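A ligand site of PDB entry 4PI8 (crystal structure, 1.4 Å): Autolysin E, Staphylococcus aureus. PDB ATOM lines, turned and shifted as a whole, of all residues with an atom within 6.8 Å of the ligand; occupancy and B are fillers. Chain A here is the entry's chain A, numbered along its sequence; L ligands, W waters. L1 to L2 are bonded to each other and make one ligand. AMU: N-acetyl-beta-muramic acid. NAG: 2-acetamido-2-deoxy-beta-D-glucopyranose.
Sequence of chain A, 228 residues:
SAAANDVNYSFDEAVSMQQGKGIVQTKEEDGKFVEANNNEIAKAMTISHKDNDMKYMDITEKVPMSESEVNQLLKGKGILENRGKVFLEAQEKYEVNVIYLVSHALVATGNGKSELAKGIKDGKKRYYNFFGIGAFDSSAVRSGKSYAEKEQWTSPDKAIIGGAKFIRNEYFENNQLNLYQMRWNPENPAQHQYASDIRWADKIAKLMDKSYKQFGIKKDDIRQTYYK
O10 of AMU L1 lies within hydrogen-bond range of OH of Tyr 171 (2.7 Å). O of Tyr 194 sits at hydrogen-bond distance from N2 of AMU L1 (2.8 Å). The backbone NH (N) of His 192 lies within hydrogen-bond range of an oxygen (O7) of NAG L2, 3.1 Å away. N of Gly 134 sits at hydrogen-bond distance from O7 of AMU L1 (2.7 Å). The backbone NH (N) of Gln 193 lies within hydrogen-bond range of an oxygen (O7) of NAG L2.
Water W6 lies within hydrogen-bond range of NE2 of His 192 (2.7 Å) and O10 of AMU L1 (2.8 Å). Water W13 lies within hydrogen-bond range of O of Ala 190 and O3 of NAG L2. Water W5 lies within hydrogen-bond range of O of Val 24 (2.7 Å) and O6 of AMU L1 (2.8 Å). Water W9 lies within hydrogen-bond range of an oxygen (O1) of AMU L1 (2.9 Å), the backbone carbonyl oxygen (O) of Gly 134 (2.9 Å) and the backbone carbonyl oxygen (O) of Gly 132 (2.9 Å). Water W1 bridges an oxygen (O6) of AMU L1 (2.9 Å) and the side-chain hydroxyl of Ser 196 (2.9 Å). Water W11 lies within hydrogen-bond range of the backbone carbonyl oxygen (O) of Gly 132 (2.9 Å), the backbone carbonyl oxygen (O) of Tyr 194 (3.0 Å) and an oxygen (O1) of AMU L1 (3.2 Å).
The backbone NH of Ala 190 lies close to the side-chain amide nitrogen of Gln 18. The side-chain amide nitrogen (NE2) of Gln 18 lies within hydrogen-bond range of the side-chain amide oxygen (OE1) of Gln 193 (2.8 Å). NE2 of Gln 193 sits close to O of Arg 183 (3.4 Å). The side-chain hydroxyl (OH) of Tyr 194 is in hydrogen-bond range of the backbone carbonyl oxygen (O) of Phe 131. The backbone carbonyl oxygen (O) of Ser 196 lies within hydrogen-bond range of the guanidinium group (NH2) of Arg 183. OE1 of Gln 193 is in hydrogen-bond range of N of Ala 190, 2.9 Å away.
Val 24 touches the ligand. O of Gly 132 touches C7 of AMU L1, 3.5 Å away. Ile 133 touches the ligand. CZ of Phe 166 touches O10 of AMU L1, 3.6 Å away. O of Ala 190 touches C8 of NAG L2 (3.3 Å). C of Gln 191 touches O7 of NAG L2, 3.6 Å away. Ser 196 touches the ligand. Hydrophobic or aromatic side chains within 4 Å of the ligand: Val 24, Phe 166, Tyr 171 and Tyr 194. Within 4 Å of the ligand: Val 24, Gly 132, Ile 133, Gly 134, Phe 166, Tyr 171, Ala 190, Gln 191, His 192, Gln 193, Tyr 194 and Ser 196.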
ATOM      1  N   GLN A  18      -7.920 -19.238  -1.399  1.00  0.00           N
ATOM      2  CA  GLN A  18      -7.845 -19.866  -0.065  1.00  0.00           C
ATOM      3  C   GLN A  18      -6.758 -20.954  -0.014  1.00  0.00           C
ATOM      4  O   GLN A  18      -6.191 -21.211   1.020  1.00  0.00           O
ATOM      5  CB  GLN A  18      -9.163 -20.494   0.291  1.00  0.00           C
ATOM      6  CG  GLN A  18     -10.315 -19.547   0.515  1.00  0.00           C
ATOM      7  CD  GLN A  18     -10.208 -18.569   1.675  1.00  0.00           C
ATOM      8  OE1 GLN A  18      -9.315 -18.708   2.513  1.00  0.00           O
ATOM      9  NE2 GLN A  18     -11.135 -17.653   1.717  1.00  0.00           N
ATOM     10  N   ILE A  23      -0.854 -19.913   3.065  1.00  0.00           N
ATOM     11  CA  ILE A  23      -2.074 -19.522   3.835  1.00  0.00           C
ATOM     12  C   ILE A  23      -2.373 -20.684   4.792  1.00  0.00           C
ATOM     13  O   ILE A  23      -2.551 -21.806   4.323  1.00  0.00           O
ATOM     14  CB  ILE A  23      -3.213 -19.206   2.920  1.00  0.00           C
ATOM     15  CG1 ILE A  23      -2.883 -17.931   2.087  1.00  0.00           C
ATOM     16  CG2 ILE A  23      -4.516 -19.045   3.712  1.00  0.00           C
ATOM     17  CD1 ILE A  23      -3.745 -17.792   0.868  1.00  0.00           C
ATOM     18  N   VAL A  24      -2.497 -20.370   6.059  1.00  0.00           N
ATOM     19  CA  VAL A  24      -2.697 -21.415   7.095  1.00  0.00           C
ATOM     20  C   VAL A  24      -4.171 -21.783   7.183  1.00  0.00           C
ATOM     21  O   VAL A  24      -5.004 -20.911   7.441  1.00  0.00           O
ATOM     22  CB  VAL A  24      -2.153 -20.961   8.440  1.00  0.00           C
ATOM     23  CG1 VAL A  24      -2.428 -22.031   9.517  1.00  0.00           C
ATOM     24  CG2 VAL A  24      -0.653 -20.641   8.331  1.00  0.00           C
ATOM     25  N   GLN A  25      -4.487 -23.038   6.918  1.00  0.00           N
ATOM     26  CA  GLN A  25      -5.839 -23.560   6.971  1.00  0.00           C
ATOM     27  C   GLN A  25      -5.703 -24.877   7.706  1.00  0.00           C
ATOM     28  O   GLN A  25      -4.955 -25.727   7.250  1.00  0.00           O
ATOM     29  CB  GLN A  25      -6.452 -23.840   5.609  1.00  0.00           C
ATOM     30  CG  GLN A  25      -6.324 -22.632   4.626  1.00  0.00           C
ATOM     31  CD  GLN A  25      -7.462 -21.664   4.653  1.00  0.00           C
ATOM     32  OE1 GLN A  25      -8.207 -21.566   5.625  1.00  0.00           O
ATOM     33  NE2 GLN A  25      -7.612 -20.867   3.614  1.00  0.00           N
ATOM     34  N   PHE A 131     -11.229 -14.447  22.869  1.00  0.00           N
ATOM     35  CA  PHE A 131     -11.730 -14.530  21.497  1.00  0.00           C
ATOM     36  C   PHE A 131     -10.657 -14.877  20.472  1.00  0.00           C
ATOM     37  O   PHE A 131     -10.851 -14.564  19.272  1.00  0.00           O
ATOM     38  CB  PHE A 131     -12.565 -13.309  21.105  1.00  0.00           C
ATOM     39  CG  PHE A 131     -13.690 -13.006  22.068  1.00  0.00           C
ATOM     40  CD1 PHE A 131     -14.912 -13.588  21.915  1.00  0.00           C
ATOM     41  CD2 PHE A 131     -13.472 -12.154  23.116  1.00  0.00           C
ATOM     42  CE1 PHE A 131     -15.962 -13.356  22.771  1.00  0.00           C
ATOM     43  CE2 PHE A 131     -14.470 -11.900  24.007  1.00  0.00           C
ATOM     44  CZ  PHE A 131     -15.720 -12.507  23.855  1.00  0.00           C
ATOM     45  N   GLY A 132      -9.540 -15.408  20.912  1.00  0.00           N
ATOM     46  CA  GLY A 132      -8.499 -15.770  19.967  1.00  0.00           C
ATOM     47  C   GLY A 132      -7.964 -14.609  19.208  1.00  0.00           C
ATOM     48  O   GLY A 132      -7.682 -14.767  17.974  1.00  0.00           O
ATOM     49  N   ILE A 133      -7.746 -13.433  19.775  1.00  0.00           N
ATOM     50  CA  ILE A 133      -7.369 -12.240  19.117  1.00  0.00           C
ATOM     51  C   ILE A 133      -5.859 -12.037  19.208  1.00  0.00           C
ATOM     52  O   ILE A 133      -5.298 -11.821  20.299  1.00  0.00           O
ATOM     53  CB  ILE A 133      -8.132 -11.007  19.638  1.00  0.00           C
ATOM     54  CG1 ILE A 133      -9.644 -11.204  19.455  1.00  0.00           C
ATOM     55  CG2 ILE A 133      -7.676  -9.725  18.985  1.00  0.00           C
ATOM     56  CD1 ILE A 133     -10.511 -10.285  20.254  1.00  0.00           C
ATOM     57  N   GLY A 134      -5.183 -12.093  18.055  1.00  0.00           N
ATOM     58  CA  GLY A 134      -3.752 -11.790  17.991  1.00  0.00           C
ATOM     59  C   GLY A 134      -2.915 -12.861  18.651  1.00  0.00           C
ATOM     60  O   GLY A 134      -3.346 -13.957  18.907  1.00  0.00           O
ATOM     61  N   ALA A 135      -1.635 -12.500  18.885  1.00  0.00           N
ATOM     62  CA  ALA A 135      -0.688 -13.389  19.484  1.00  0.00           C
ATOM     63  C   ALA A 135      -0.877 -13.352  21.006  1.00  0.00           C
ATOM     64  O   ALA A 135      -0.939 -12.256  21.594  1.00  0.00           O
ATOM     65  CB  ALA A 135       0.740 -13.000  19.095  1.00  0.00           C
ATOM     66  N   PHE A 166     -13.333  -5.156  19.601  1.00  0.00           N
ATOM     67  CA  PHE A 166     -12.491  -5.593  18.477  1.00  0.00           C
ATOM     68  C   PHE A 166     -13.369  -6.200  17.358  1.00  0.00           C
ATOM     69  O   PHE A 166     -13.252  -5.846  16.155  1.00  0.00           O
ATOM     70  CB  PHE A 166     -11.490  -6.579  18.946  1.00  0.00           C
ATOM     71  CG  PHE A 166     -10.678  -7.226  17.827  1.00  0.00           C
ATOM     72  CD1 PHE A 166      -9.557  -6.602  17.314  1.00  0.00           C
ATOM     73  CD2 PHE A 166     -11.061  -8.427  17.295  1.00  0.00           C
ATOM     74  CE1 PHE A 166      -8.809  -7.223  16.292  1.00  0.00           C
ATOM     75  CE2 PHE A 166     -10.311  -9.033  16.290  1.00  0.00           C
ATOM     76  CZ  PHE A 166      -9.198  -8.408  15.799  1.00  0.00           C
ATOM     77  N   GLU A 170     -13.334  -4.187  13.968  1.00  0.00           N
ATOM     78  CA  GLU A 170     -12.477  -4.739  12.928  1.00  0.00           C
ATOM     79  C   GLU A 170     -13.165  -5.671  11.946  1.00  0.00           C
ATOM     80  O   GLU A 170     -12.719  -5.800  10.816  1.00  0.00           O
ATOM     81  CB  GLU A 170     -11.278  -5.458  13.513  1.00  0.00           C
ATOM     82  CG  GLU A 170     -10.521  -4.544  14.472  1.00  0.00           C
ATOM     83  CD  GLU A 170     -10.071  -3.246  13.842  1.00  0.00           C
ATOM     84  OE1 GLU A 170      -9.621  -3.270  12.657  1.00  0.00           O
ATOM     85  OE2 GLU A 170     -10.185  -2.211  14.547  1.00  0.00           O
ATOM     86  N   TYR A 171     -14.248  -6.352  12.352  1.00  0.00           N
ATOM     87  CA  TYR A 171     -14.989  -7.266  11.503  1.00  0.00           C
ATOM     88  C   TYR A 171     -16.320  -6.673  11.093  1.00  0.00           C
ATOM     89  O   TYR A 171     -16.638  -6.528   9.879  1.00  0.00           O
ATOM     90  CB  TYR A 171     -15.105  -8.677  12.145  1.00  0.00           C
ATOM     91  CG  TYR A 171     -13.803  -9.407  12.015  1.00  0.00           C
ATOM     92  CD1 TYR A 171     -12.743  -9.162  12.897  1.00  0.00           C
ATOM     93  CD2 TYR A 171     -13.567 -10.290  10.972  1.00  0.00           C
ATOM     94  CE1 TYR A 171     -11.501  -9.761  12.774  1.00  0.00           C
ATOM     95  CE2 TYR A 171     -12.301 -10.872  10.826  1.00  0.00           C
ATOM     96  CZ  TYR A 171     -11.306 -10.617  11.719  1.00  0.00           C
ATOM     97  OH  TYR A 171     -10.077 -11.202  11.538  1.00  0.00           O
ATOM     98  N   ARG A 183     -14.970 -15.840   8.603  1.00  0.00           N
ATOM     99  CA  ARG A 183     -14.042 -16.912   8.369  1.00  0.00           C
ATOM    100  C   ARG A 183     -13.417 -16.917   6.954  1.00  0.00           C
ATOM    101  O   ARG A 183     -12.263 -17.276   6.790  1.00  0.00           O
ATOM    102  CB  ARG A 183     -14.706 -18.266   8.652  1.00  0.00           C
ATOM    103  CG  ARG A 183     -13.839 -19.472   8.380  1.00  0.00           C
ATOM    104  CD  ARG A 183     -12.534 -19.500   9.185  1.00  0.00           C
ATOM    105  NE  ARG A 183     -11.695 -20.653   8.859  1.00  0.00           N
ATOM    106  CZ  ARG A 183     -10.860 -20.708   7.829  1.00  0.00           C
ATOM    107  NH1 ARG A 183     -10.800 -19.731   6.944  1.00  0.00           N
ATOM    108  NH2 ARG A 183     -10.101 -21.796   7.675  1.00  0.00           N
ATOM    109  N   ALA A 190      -9.221 -14.831   1.418  1.00  0.00           N
ATOM    110  CA  ALA A 190      -7.935 -15.156   1.982  1.00  0.00           C
ATOM    111  C   ALA A 190      -7.259 -14.022   2.704  1.00  0.00           C
ATOM    112  O   ALA A 190      -6.071 -14.157   3.118  1.00  0.00           O
ATOM    113  CB  ALA A 190      -6.987 -15.856   0.965  1.00  0.00           C
ATOM    114  N   GLN A 191      -7.908 -12.885   2.899  1.00  0.00           N
ATOM    115  CA  GLN A 191      -7.442 -11.797   3.701  1.00  0.00           C
ATOM    116  C   GLN A 191      -8.381 -11.652   4.861  1.00  0.00           C
ATOM    117  O   GLN A 191      -9.589 -11.793   4.731  1.00  0.00           O
ATOM    118  CB  GLN A 191      -7.551 -10.413   2.919  1.00  0.00           C
ATOM    119  CG  GLN A 191      -6.645 -10.397   1.743  1.00  0.00           C
ATOM    120  CD  GLN A 191      -6.508  -9.000   1.222  1.00  0.00           C
ATOM    121  OE1 GLN A 191      -7.000  -8.683   0.141  1.00  0.00           O
ATOM    122  NE2 GLN A 191      -5.902  -8.169   2.004  1.00  0.00           N
ATOM    123  N   HIS A 192      -7.831 -11.119   5.949  1.00  0.00           N
ATOM    124  CA  HIS A 192      -8.607 -10.677   7.097  1.00  0.00           C
ATOM    125  C   HIS A 192      -9.607 -11.742   7.537  1.00  0.00           C
ATOM    126  O   HIS A 192     -10.800 -11.418   7.759  1.00  0.00           O
ATOM    127  CB  HIS A 192      -9.284  -9.318   6.864  1.00  0.00           C
ATOM    128  CG  HIS A 192      -9.586  -8.634   8.160  1.00  0.00           C
ATOM    129  ND1 HIS A 192     -10.861  -8.563   8.677  1.00  0.00           N
ATOM    130  CD2 HIS A 192      -8.754  -8.160   9.120  1.00  0.00           C
ATOM    131  CE1 HIS A 192     -10.810  -8.019   9.876  1.00  0.00           C
ATOM    132  NE2 HIS A 192      -9.545  -7.775  10.188  1.00  0.00           N
ATOM    133  N   GLN A 193      -9.119 -12.930   7.775  1.00  0.00           N
ATOM    134  CA  GLN A 193      -9.981 -14.072   8.218  1.00  0.00           C
ATOM    135  C   GLN A 193      -9.716 -14.353   9.672  1.00  0.00           C
ATOM    136  O   GLN A 193      -8.613 -14.352  10.179  1.00  0.00           O
ATOM    137  CB  GLN A 193      -9.714 -15.263   7.328  1.00  0.00           C
ATOM    138  CG  GLN A 193     -10.243 -14.970   5.935  1.00  0.00           C
ATOM    139  CD  GLN A 193     -10.093 -15.999   4.819  1.00  0.00           C
ATOM    140  OE1 GLN A 193     -10.665 -15.769   3.768  1.00  0.00           O
ATOM    141  NE2 GLN A 193      -9.358 -17.045   5.027  1.00  0.00           N
ATOM    142  N   TYR A 194     -10.818 -14.682  10.375  1.00  0.00           N
ATOM    143  CA  TYR A 194     -10.726 -14.680  11.848  1.00  0.00           C
ATOM    144  C   TYR A 194      -9.935 -15.827  12.371  1.00  0.00           C
ATOM    145  O   TYR A 194      -9.323 -15.718  13.454  1.00  0.00           O
ATOM    146  CB  TYR A 194     -12.152 -14.671  12.446  1.00  0.00           C
ATOM    147  CG  TYR A 194     -12.160 -14.112  13.893  1.00  0.00           C
ATOM    148  CD1 TYR A 194     -11.806 -14.945  14.969  1.00  0.00           C
ATOM    149  CD2 TYR A 194     -12.501 -12.833  14.145  1.00  0.00           C
ATOM    150  CE1 TYR A 194     -11.710 -14.399  16.232  1.00  0.00           C
ATOM    151  CE2 TYR A 194     -12.407 -12.300  15.443  1.00  0.00           C
ATOM    152  CZ  TYR A 194     -12.016 -13.112  16.444  1.00  0.00           C
ATOM    153  OH  TYR A 194     -11.967 -12.544  17.741  1.00  0.00           O
ATOM    154  N   ALA A 195      -9.966 -16.976  11.696  1.00  0.00           N
ATOM    155  CA  ALA A 195      -9.371 -18.165  12.213  1.00  0.00           C
ATOM    156  C   ALA A 195      -8.846 -19.049  11.109  1.00  0.00           C
ATOM    157  O   ALA A 195      -9.337 -18.927   9.969  1.00  0.00           O
ATOM    158  CB  ALA A 195     -10.402 -18.902  13.025  1.00  0.00           C
ATOM    159  N   SER A 196      -7.878 -19.933  11.436  1.00  0.00           N
ATOM    160  CA  SER A 196      -7.407 -20.948  10.480  1.00  0.00           C
ATOM    161  C   SER A 196      -8.179 -22.222  10.500  1.00  0.00           C
ATOM    162  O   SER A 196      -8.201 -22.936   9.525  1.00  0.00           O
ATOM    163  CB  SER A 196      -5.923 -21.197  10.674  1.00  0.00           C
ATOM    164  OG  SER A 196      -5.666 -21.804  11.928  1.00  0.00           O
HETATM  165  C1  AMU L   1      -5.993 -16.057  13.426  1.00  0.00           C
HETATM  166  C2  AMU L   1      -5.941 -14.560  13.555  1.00  0.00           C
HETATM  167  C3  AMU L   1      -5.800 -13.922  12.159  1.00  0.00           C
HETATM  168  C4  AMU L   1      -4.575 -14.555  11.454  1.00  0.00           C
HETATM  169  C5  AMU L   1      -4.658 -16.049  11.545  1.00  0.00           C
HETATM  170  C6  AMU L   1      -3.443 -16.715  10.886  1.00  0.00           C
HETATM  171  C7  AMU L   1      -7.209 -12.993  15.038  1.00  0.00           C
HETATM  172  C8  AMU L   1      -8.599 -12.558  15.429  1.00  0.00           C
HETATM  173  C9  AMU L   1      -6.825 -11.764  11.821  1.00  0.00           C
HETATM  174  C10 AMU L   1      -6.907 -10.504  12.590  1.00  0.00           C
HETATM  175  C11 AMU L   1      -6.754 -11.504  10.325  1.00  0.00           C
HETATM  176  O1  AMU L   1      -6.075 -16.671  14.706  1.00  0.00           O
HETATM  177  O3  AMU L   1      -5.672 -12.502  12.239  1.00  0.00           O
HETATM  178  O4  AMU L   1      -4.645 -14.057  10.106  1.00  0.00           O
HETATM  179  O5  AMU L   1      -4.737 -16.462  12.889  1.00  0.00           O
HETATM  180  O6  AMU L   1      -3.587 -18.134  10.784  1.00  0.00           O
HETATM  181  O7  AMU L   1      -6.218 -12.518  15.555  1.00  0.00           O
HETATM  182  O10 AMU L   1      -8.038  -9.954  12.778  1.00  0.00           O
HETATM  183  O11 AMU L   1      -5.817  -9.953  13.002  1.00  0.00           O
HETATM  184  N2  AMU L   1      -7.172 -14.007  14.181  1.00  0.00           N
HETATM  185  C1  NAG L   2      -3.414 -13.556   9.620  1.00  0.00           C
HETATM  186  C2  NAG L   2      -3.723 -13.239   8.147  1.00  0.00           C
HETATM  187  C3  NAG L   2      -2.454 -12.662   7.503  1.00  0.00           C
HETATM  188  C4  NAG L   2      -1.996 -11.514   8.350  1.00  0.00           C
HETATM  189  C5  NAG L   2      -1.823 -11.889   9.817  1.00  0.00           C
HETATM  190  C6  NAG L   2      -1.581 -10.640  10.612  1.00  0.00           C
HETATM  191  C7  NAG L   2      -5.522 -14.458   6.908  1.00  0.00           C
HETATM  192  C8  NAG L   2      -5.839 -15.654   6.099  1.00  0.00           C
HETATM  193  N2  NAG L   2      -4.258 -14.346   7.357  1.00  0.00           N
HETATM  194  O3  NAG L   2      -2.788 -12.188   6.205  1.00  0.00           O
HETATM  195  O4  NAG L   2      -0.705 -11.107   7.901  1.00  0.00           O
HETATM  196  O5  NAG L   2      -3.066 -12.381  10.320  1.00  0.00           O
HETATM  197  O6  NAG L   2      -1.266 -11.125  11.922  1.00  0.00           O
HETATM  198  O7  NAG L   2      -6.364 -13.585   7.155  1.00  0.00           O
HETATM  199  O   HOH W   1      -3.898 -19.817  13.135  1.00  0.00           O
HETATM  200  O   HOH W   2      -7.041 -16.683   9.384  1.00  0.00           O
HETATM  201  O   HOH W   3      -5.651  -7.916  14.810  1.00  0.00           O
HETATM  202  O   HOH W   4      -0.497 -11.368   4.941  1.00  0.00           O
HETATM  203  O   HOH W   5      -5.071 -18.426   8.386  1.00  0.00           O
HETATM  204  O   HOH W   6      -8.360  -7.210  12.553  1.00  0.00           O
HETATM  205  O   HOH W   7      -1.595  -8.102   7.363  1.00  0.00           O
HETATM  206  O   HOH W   8      -3.582 -11.420  13.732  1.00  0.00           O
HETATM  207  O   HOH W   9      -4.981 -15.514  17.084  1.00  0.00           O
HETATM  208  O   HOH W  10       1.316 -13.896   8.000  1.00  0.00           O
HETATM  209  O   HOH W  11      -8.876 -16.723  16.205  1.00  0.00           O
HETATM  210  O   HOH W  12      -4.360  -8.336  11.270  1.00  0.00           O
HETATM  211  O   HOH W  13      -3.554 -13.577   3.895  1.00  0.00           O
